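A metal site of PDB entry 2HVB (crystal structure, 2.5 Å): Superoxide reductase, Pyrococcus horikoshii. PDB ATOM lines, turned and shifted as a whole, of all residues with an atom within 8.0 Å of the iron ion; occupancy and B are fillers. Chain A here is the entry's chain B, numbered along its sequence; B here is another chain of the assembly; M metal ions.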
ATOM      1  N   TRP A  20       5.915 -36.409  -6.458  1.00  0.00           N
ATOM      2  CA  TRP A  20       5.196 -37.156  -5.438  1.00  0.00           C
ATOM      3  C   TRP A  20       3.982 -36.275  -5.163  1.00  0.00           C
ATOM      4  O   TRP A  20       4.069 -35.060  -5.297  1.00  0.00           O
ATOM      5  CB  TRP A  20       6.080 -37.348  -4.183  1.00  0.00           C
ATOM      6  CG  TRP A  20       6.494 -36.114  -3.445  1.00  0.00           C
ATOM      7  CD1 TRP A  20       5.680 -35.256  -2.775  1.00  0.00           C
ATOM      8  CD2 TRP A  20       7.823 -35.625  -3.275  1.00  0.00           C
ATOM      9  NE1 TRP A  20       6.421 -34.260  -2.187  1.00  0.00           N
ATOM     10  CE2 TRP A  20       7.744 -34.456  -2.483  1.00  0.00           C
ATOM     11  CE3 TRP A  20       9.084 -36.058  -3.708  1.00  0.00           C
ATOM     12  CZ2 TRP A  20       8.870 -33.719  -2.113  1.00  0.00           C
ATOM     13  CZ3 TRP A  20      10.210 -35.322  -3.338  1.00  0.00           C
ATOM     14  CH2 TRP A  20      10.097 -34.167  -2.554  1.00  0.00           C
ATOM     15  N   GLU A  23       3.248 -31.698  -4.484  1.00  0.00           N
ATOM     16  CA  GLU A  23       4.295 -30.682  -4.688  1.00  0.00           C
ATOM     17  C   GLU A  23       4.951 -30.823  -6.053  1.00  0.00           C
ATOM     18  O   GLU A  23       5.459 -31.871  -6.429  1.00  0.00           O
ATOM     19  CB  GLU A  23       5.407 -30.834  -3.666  1.00  0.00           C
ATOM     20  CG  GLU A  23       5.838 -29.473  -3.103  1.00  0.00           C
ATOM     21  CD  GLU A  23       6.925 -29.681  -2.074  1.00  0.00           C
ATOM     22  OE1 GLU A  23       6.610 -30.085  -0.963  1.00  0.00           O
ATOM     23  OE2 GLU A  23       8.084 -29.422  -2.391  1.00  0.00           O
ATOM     24  N   LYS A  24       4.898 -29.723  -6.821  1.00  0.00           N
ATOM     25  CA  LYS A  24       5.581 -29.758  -8.104  1.00  0.00           C
ATOM     26  C   LYS A  24       7.087 -29.494  -7.952  1.00  0.00           C
ATOM     27  O   LYS A  24       7.507 -28.557  -7.283  1.00  0.00           O
ATOM     28  CB  LYS A  24       4.942 -28.733  -9.029  1.00  0.00           C
ATOM     29  CG  LYS A  24       3.847 -29.357  -9.907  1.00  0.00           C
ATOM     30  CD  LYS A  24       2.963 -30.335  -9.141  1.00  0.00           C
ATOM     31  CE  LYS A  24       1.792 -30.855  -9.978  1.00  0.00           C
ATOM     32  NZ  LYS A  24       2.274 -31.806 -10.972  1.00  0.00           N
ATOM     33  N   HIS A  25       7.903 -30.322  -8.607  1.00  0.00           N
ATOM     34  CA  HIS A  25       9.352 -30.148  -8.616  1.00  0.00           C
ATOM     35  C   HIS A  25       9.883 -30.341 -10.027  1.00  0.00           C
ATOM     36  O   HIS A  25      10.842 -29.681 -10.431  1.00  0.00           O
ATOM     37  CB  HIS A  25      10.041 -31.170  -7.726  1.00  0.00           C
ATOM     38  CG  HIS A  25       9.984 -30.846  -6.261  1.00  0.00           C
ATOM     39  ND1 HIS A  25       9.420 -31.696  -5.342  1.00  0.00           N
ATOM     40  CD2 HIS A  25      10.480 -29.801  -5.562  1.00  0.00           C
ATOM     41  CE1 HIS A  25       9.575 -31.190  -4.125  1.00  0.00           C
ATOM     42  NE2 HIS A  25      10.213 -30.039  -4.232  1.00  0.00           N
ATOM     43  N   VAL A  44       8.841 -24.300 -12.735  1.00  0.00           N
ATOM     44  CA  VAL A  44       8.472 -25.311 -11.760  1.00  0.00           C
ATOM     45  C   VAL A  44       7.175 -24.891 -11.077  1.00  0.00           C
ATOM     46  O   VAL A  44       7.135 -23.899 -10.345  1.00  0.00           O
ATOM     47  CB  VAL A  44       9.610 -25.531 -10.700  1.00  0.00           C
ATOM     48  CG1 VAL A  44       9.114 -26.454  -9.544  1.00  0.00           C
ATOM     49  CG2 VAL A  44      10.831 -26.156 -11.387  1.00  0.00           C
ATOM     50  N   HIS A  50       4.998 -24.176  -6.249  1.00  0.00           N
ATOM     51  CA  HIS A  50       5.825 -24.897  -5.294  1.00  0.00           C
ATOM     52  C   HIS A  50       6.091 -23.857  -4.203  1.00  0.00           C
ATOM     53  O   HIS A  50       6.088 -22.667  -4.482  1.00  0.00           O
ATOM     54  CB  HIS A  50       7.102 -25.346  -5.996  1.00  0.00           C
ATOM     55  CG  HIS A  50       8.166 -25.825  -5.070  1.00  0.00           C
ATOM     56  ND1 HIS A  50       8.856 -24.964  -4.237  1.00  0.00           N
ATOM     57  CD2 HIS A  50       8.635 -27.066  -4.802  1.00  0.00           C
ATOM     58  CE1 HIS A  50       9.712 -25.668  -3.509  1.00  0.00           C
ATOM     59  NE2 HIS A  50       9.592 -26.936  -3.833  1.00  0.00           N
ATOM     60  N   PRO A  51       6.307 -24.287  -2.956  1.00  0.00           N
ATOM     61  CA  PRO A  51       6.558 -23.281  -1.924  1.00  0.00           C
ATOM     62  C   PRO A  51       7.745 -22.379  -2.262  1.00  0.00           C
ATOM     63  O   PRO A  51       8.769 -22.856  -2.748  1.00  0.00           O
ATOM     64  CB  PRO A  51       6.815 -24.109  -0.666  1.00  0.00           C
ATOM     65  CG  PRO A  51       6.493 -25.520  -0.962  1.00  0.00           C
ATOM     66  CD  PRO A  51       6.125 -25.644  -2.415  1.00  0.00           C
ATOM     67  N   HIS A  56      12.294 -22.693   2.111  1.00  0.00           N
ATOM     68  CA  HIS A  56      11.991 -23.690   1.096  1.00  0.00           C
ATOM     69  C   HIS A  56      11.679 -23.030  -0.224  1.00  0.00           C
ATOM     70  O   HIS A  56      10.780 -22.185  -0.301  1.00  0.00           O
ATOM     71  CB  HIS A  56      10.795 -24.526   1.552  1.00  0.00           C
ATOM     72  CG  HIS A  56      10.489 -25.690   0.657  1.00  0.00           C
ATOM     73  ND1 HIS A  56       9.327 -26.421   0.762  1.00  0.00           N
ATOM     74  CD2 HIS A  56      11.200 -26.249  -0.359  1.00  0.00           C
ATOM     75  CE1 HIS A  56       9.330 -27.377  -0.138  1.00  0.00           C
ATOM     76  NE2 HIS A  56      10.449 -27.299  -0.831  1.00  0.00           N
ATOM     77  N   HIS A  57      12.391 -23.422  -1.271  1.00  0.00           N
ATOM     78  CA  HIS A  57      12.150 -22.835  -2.593  1.00  0.00           C
ATOM     79  C   HIS A  57      12.923 -23.553  -3.719  1.00  0.00           C
ATOM     80  O   HIS A  57      13.705 -24.468  -3.478  1.00  0.00           O
ATOM     81  CB  HIS A  57      12.571 -21.361  -2.540  1.00  0.00           C
ATOM     82  CG  HIS A  57      13.993 -21.251  -2.057  1.00  0.00           C
ATOM     83  ND1 HIS A  57      14.318 -20.852  -0.803  1.00  0.00           N
ATOM     84  CD2 HIS A  57      15.168 -21.515  -2.757  1.00  0.00           C
ATOM     85  CE1 HIS A  57      15.665 -20.877  -0.755  1.00  0.00           C
ATOM     86  NE2 HIS A  57      16.201 -21.275  -1.910  1.00  0.00           N
ATOM     87  N   ILE A  58      12.625 -23.149  -4.950  1.00  0.00           N
ATOM     88  CA  ILE A  58      13.303 -23.707  -6.125  1.00  0.00           C
ATOM     89  C   ILE A  58      14.412 -22.658  -6.339  1.00  0.00           C
ATOM     90  O   ILE A  58      14.134 -21.493  -6.638  1.00  0.00           O
ATOM     91  CB  ILE A  58      12.358 -23.738  -7.348  1.00  0.00           C
ATOM     92  CG1 ILE A  58      11.196 -24.704  -7.083  1.00  0.00           C
ATOM     93  CG2 ILE A  58      13.127 -24.154  -8.586  1.00  0.00           C
ATOM     94  CD1 ILE A  58      11.607 -26.166  -6.919  1.00  0.00           C
ATOM     95  N   TYR A 110      16.708 -27.435  -9.001  1.00  0.00           N
ATOM     96  CA  TYR A 110      17.070 -27.707  -7.619  1.00  0.00           C
ATOM     97  C   TYR A 110      16.218 -27.043  -6.562  1.00  0.00           C
ATOM     98  O   TYR A 110      16.033 -25.825  -6.549  1.00  0.00           O
ATOM     99  CB  TYR A 110      18.526 -27.314  -7.384  1.00  0.00           C
ATOM    100  CG  TYR A 110      19.019 -27.499  -5.954  1.00  0.00           C
ATOM    101  CD1 TYR A 110      19.290 -28.774  -5.453  1.00  0.00           C
ATOM    102  CD2 TYR A 110      19.226 -26.410  -5.117  1.00  0.00           C
ATOM    103  CE1 TYR A 110      19.741 -28.948  -4.147  1.00  0.00           C
ATOM    104  CE2 TYR A 110      19.682 -26.576  -3.807  1.00  0.00           C
ATOM    105  CZ  TYR A 110      19.938 -27.846  -3.339  1.00  0.00           C
ATOM    106  OH  TYR A 110      20.389 -28.020  -2.033  1.00  0.00           O
ATOM    107  N   CYS A 111      15.698 -27.859  -5.656  1.00  0.00           N
ATOM    108  CA  CYS A 111      14.922 -27.361  -4.541  1.00  0.00           C
ATOM    109  C   CYS A 111      15.926 -27.429  -3.392  1.00  0.00           C
ATOM    110  O   CYS A 111      16.618 -28.434  -3.215  1.00  0.00           O
ATOM    111  CB  CYS A 111      13.731 -28.292  -4.282  1.00  0.00           C
ATOM    112  SG  CYS A 111      12.781 -27.840  -2.829  1.00  0.00           S
ATOM    113  N   ASN A 112      16.033 -26.364  -2.606  1.00  0.00           N
ATOM    114  CA  ASN A 112      17.021 -26.396  -1.540  1.00  0.00           C
ATOM    115  C   ASN A 112      16.846 -27.465  -0.459  1.00  0.00           C
ATOM    116  O   ASN A 112      17.733 -27.652   0.358  1.00  0.00           O
ATOM    117  CB  ASN A 112      17.154 -25.016  -0.894  1.00  0.00           C
ATOM    118  CG  ASN A 112      15.931 -24.623  -0.094  1.00  0.00           C
ATOM    119  OD1 ASN A 112      14.805 -24.908  -0.495  1.00  0.00           O
ATOM    120  ND2 ASN A 112      16.144 -23.975   1.053  1.00  0.00           N
ATOM    121  N   ILE A 113      15.732 -28.177  -0.453  1.00  0.00           N
ATOM    122  CA  ILE A 113      15.536 -29.233   0.542  1.00  0.00           C
ATOM    123  C   ILE A 113      15.051 -30.540  -0.072  1.00  0.00           C
ATOM    124  O   ILE A 113      14.995 -31.553   0.607  1.00  0.00           O
ATOM    125  CB  ILE A 113      14.506 -28.851   1.653  1.00  0.00           C
ATOM    126  CG1 ILE A 113      13.128 -28.590   1.030  1.00  0.00           C
ATOM    127  CG2 ILE A 113      15.013 -27.635   2.453  1.00  0.00           C
ATOM    128  CD1 ILE A 113      11.997 -28.476   2.070  1.00  0.00           C
ATOM    129  N   HIS A 114      14.701 -30.515  -1.353  1.00  0.00           N
ATOM    130  CA  HIS A 114      14.208 -31.693  -2.035  1.00  0.00           C
ATOM    131  C   HIS A 114      15.105 -32.153  -3.184  1.00  0.00           C
ATOM    132  O   HIS A 114      14.716 -32.969  -4.012  1.00  0.00           O
ATOM    133  CB  HIS A 114      12.786 -31.449  -2.524  1.00  0.00           C
ATOM    134  CG  HIS A 114      11.800 -31.296  -1.415  1.00  0.00           C
ATOM    135  ND1 HIS A 114      10.806 -30.342  -1.416  1.00  0.00           N
ATOM    136  CD2 HIS A 114      11.652 -31.975  -0.253  1.00  0.00           C
ATOM    137  CE1 HIS A 114      10.100 -30.436  -0.311  1.00  0.00           C
ATOM    138  NE2 HIS A 114      10.591 -31.426   0.411  1.00  0.00           N
ATOM    139  N   GLY A 115      16.322 -31.609  -3.222  1.00  0.00           N
ATOM    140  CA  GLY A 115      17.297 -31.994  -4.228  1.00  0.00           C
ATOM    141  C   GLY A 115      17.077 -31.646  -5.684  1.00  0.00           C
ATOM    142  O   GLY A 115      16.341 -30.726  -6.024  1.00  0.00           O
ATOM    143  N   TRP A 117      16.111 -32.324  -9.765  1.00  0.00           N
ATOM    144  CA  TRP A 117      15.032 -32.858 -10.588  1.00  0.00           C
ATOM    145  C   TRP A 117      15.337 -32.612 -12.058  1.00  0.00           C
ATOM    146  O   TRP A 117      16.071 -31.689 -12.412  1.00  0.00           O
ATOM    147  CB  TRP A 117      13.694 -32.203 -10.235  1.00  0.00           C
ATOM    148  CG  TRP A 117      13.274 -32.467  -8.833  1.00  0.00           C
ATOM    149  CD1 TRP A 117      13.787 -31.911  -7.699  1.00  0.00           C
ATOM    150  CD2 TRP A 117      12.286 -33.394  -8.403  1.00  0.00           C
ATOM    151  NE1 TRP A 117      13.177 -32.432  -6.593  1.00  0.00           N
ATOM    152  CE2 TRP A 117      12.248 -33.359  -6.992  1.00  0.00           C
ATOM    153  CE3 TRP A 117      11.416 -34.267  -9.075  1.00  0.00           C
ATOM    154  CZ2 TRP A 117      11.385 -34.153  -6.238  1.00  0.00           C
ATOM    155  CZ3 TRP A 117      10.552 -35.062  -8.321  1.00  0.00           C
ATOM    156  CH2 TRP A 117      10.539 -34.999  -6.915  1.00  0.00           C
ATOM    157  N   PHE B  72      17.734 -36.395   0.536  1.00  0.00           N
ATOM    158  CA  PHE B  72      18.205 -35.583  -0.591  1.00  0.00           C
ATOM    159  C   PHE B  72      19.635 -35.042  -0.372  1.00  0.00           C
ATOM    160  O   PHE B  72      20.016 -34.643   0.719  1.00  0.00           O
ATOM    161  CB  PHE B  72      17.231 -34.428  -0.802  1.00  0.00           C
ATOM    162  CG  PHE B  72      15.838 -34.957  -0.951  1.00  0.00           C
ATOM    163  CD1 PHE B  72      15.403 -35.403  -2.189  1.00  0.00           C
ATOM    164  CD2 PHE B  72      14.985 -34.977   0.146  1.00  0.00           C
ATOM    165  CE1 PHE B  72      14.098 -35.869  -2.335  1.00  0.00           C
ATOM    166  CE2 PHE B  72      13.683 -35.452  -0.011  1.00  0.00           C
ATOM    167  CZ  PHE B  72      13.236 -35.890  -1.248  1.00  0.00           C
HETATM  168 FE    FE M   1      10.465 -28.720  -2.609  1.00  0.00          FE
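The iron ion is bound by a ring nitrogen (ND1) of His 114 (2.0 Å), a ring nitrogen (NE2) of His 25 (2.1 Å), a ring nitrogen (NE2) of His 56 (2.3 Å), a ring nitrogen (NE2) of His 50 (2.3 Å), the side-chain sulfur of Cys 111 (2.5 Å) and the side-chain carboxylate of Glu 23 (2.5 Å).
The iron ion has six donor atoms within binding distance.
Six residues have an atom within 4 Å of the iron ion: Glu 23, His 25, His 50, His 56, Cys 111 and His 114.
The nearest printed residue that does not touch the iron ion is Ile 113 (4.5 Å).
The side-chain sulfur (SG) of Cys 111 sits close to the backbone carbonyl oxygen (O) of His 57 (3.6 Å).
The backbone carbonyl oxygen (O) of His 114 is in hydrogen-bond range of the indole nitrogen (NE1) of Trp 117, at 3.1 Å.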
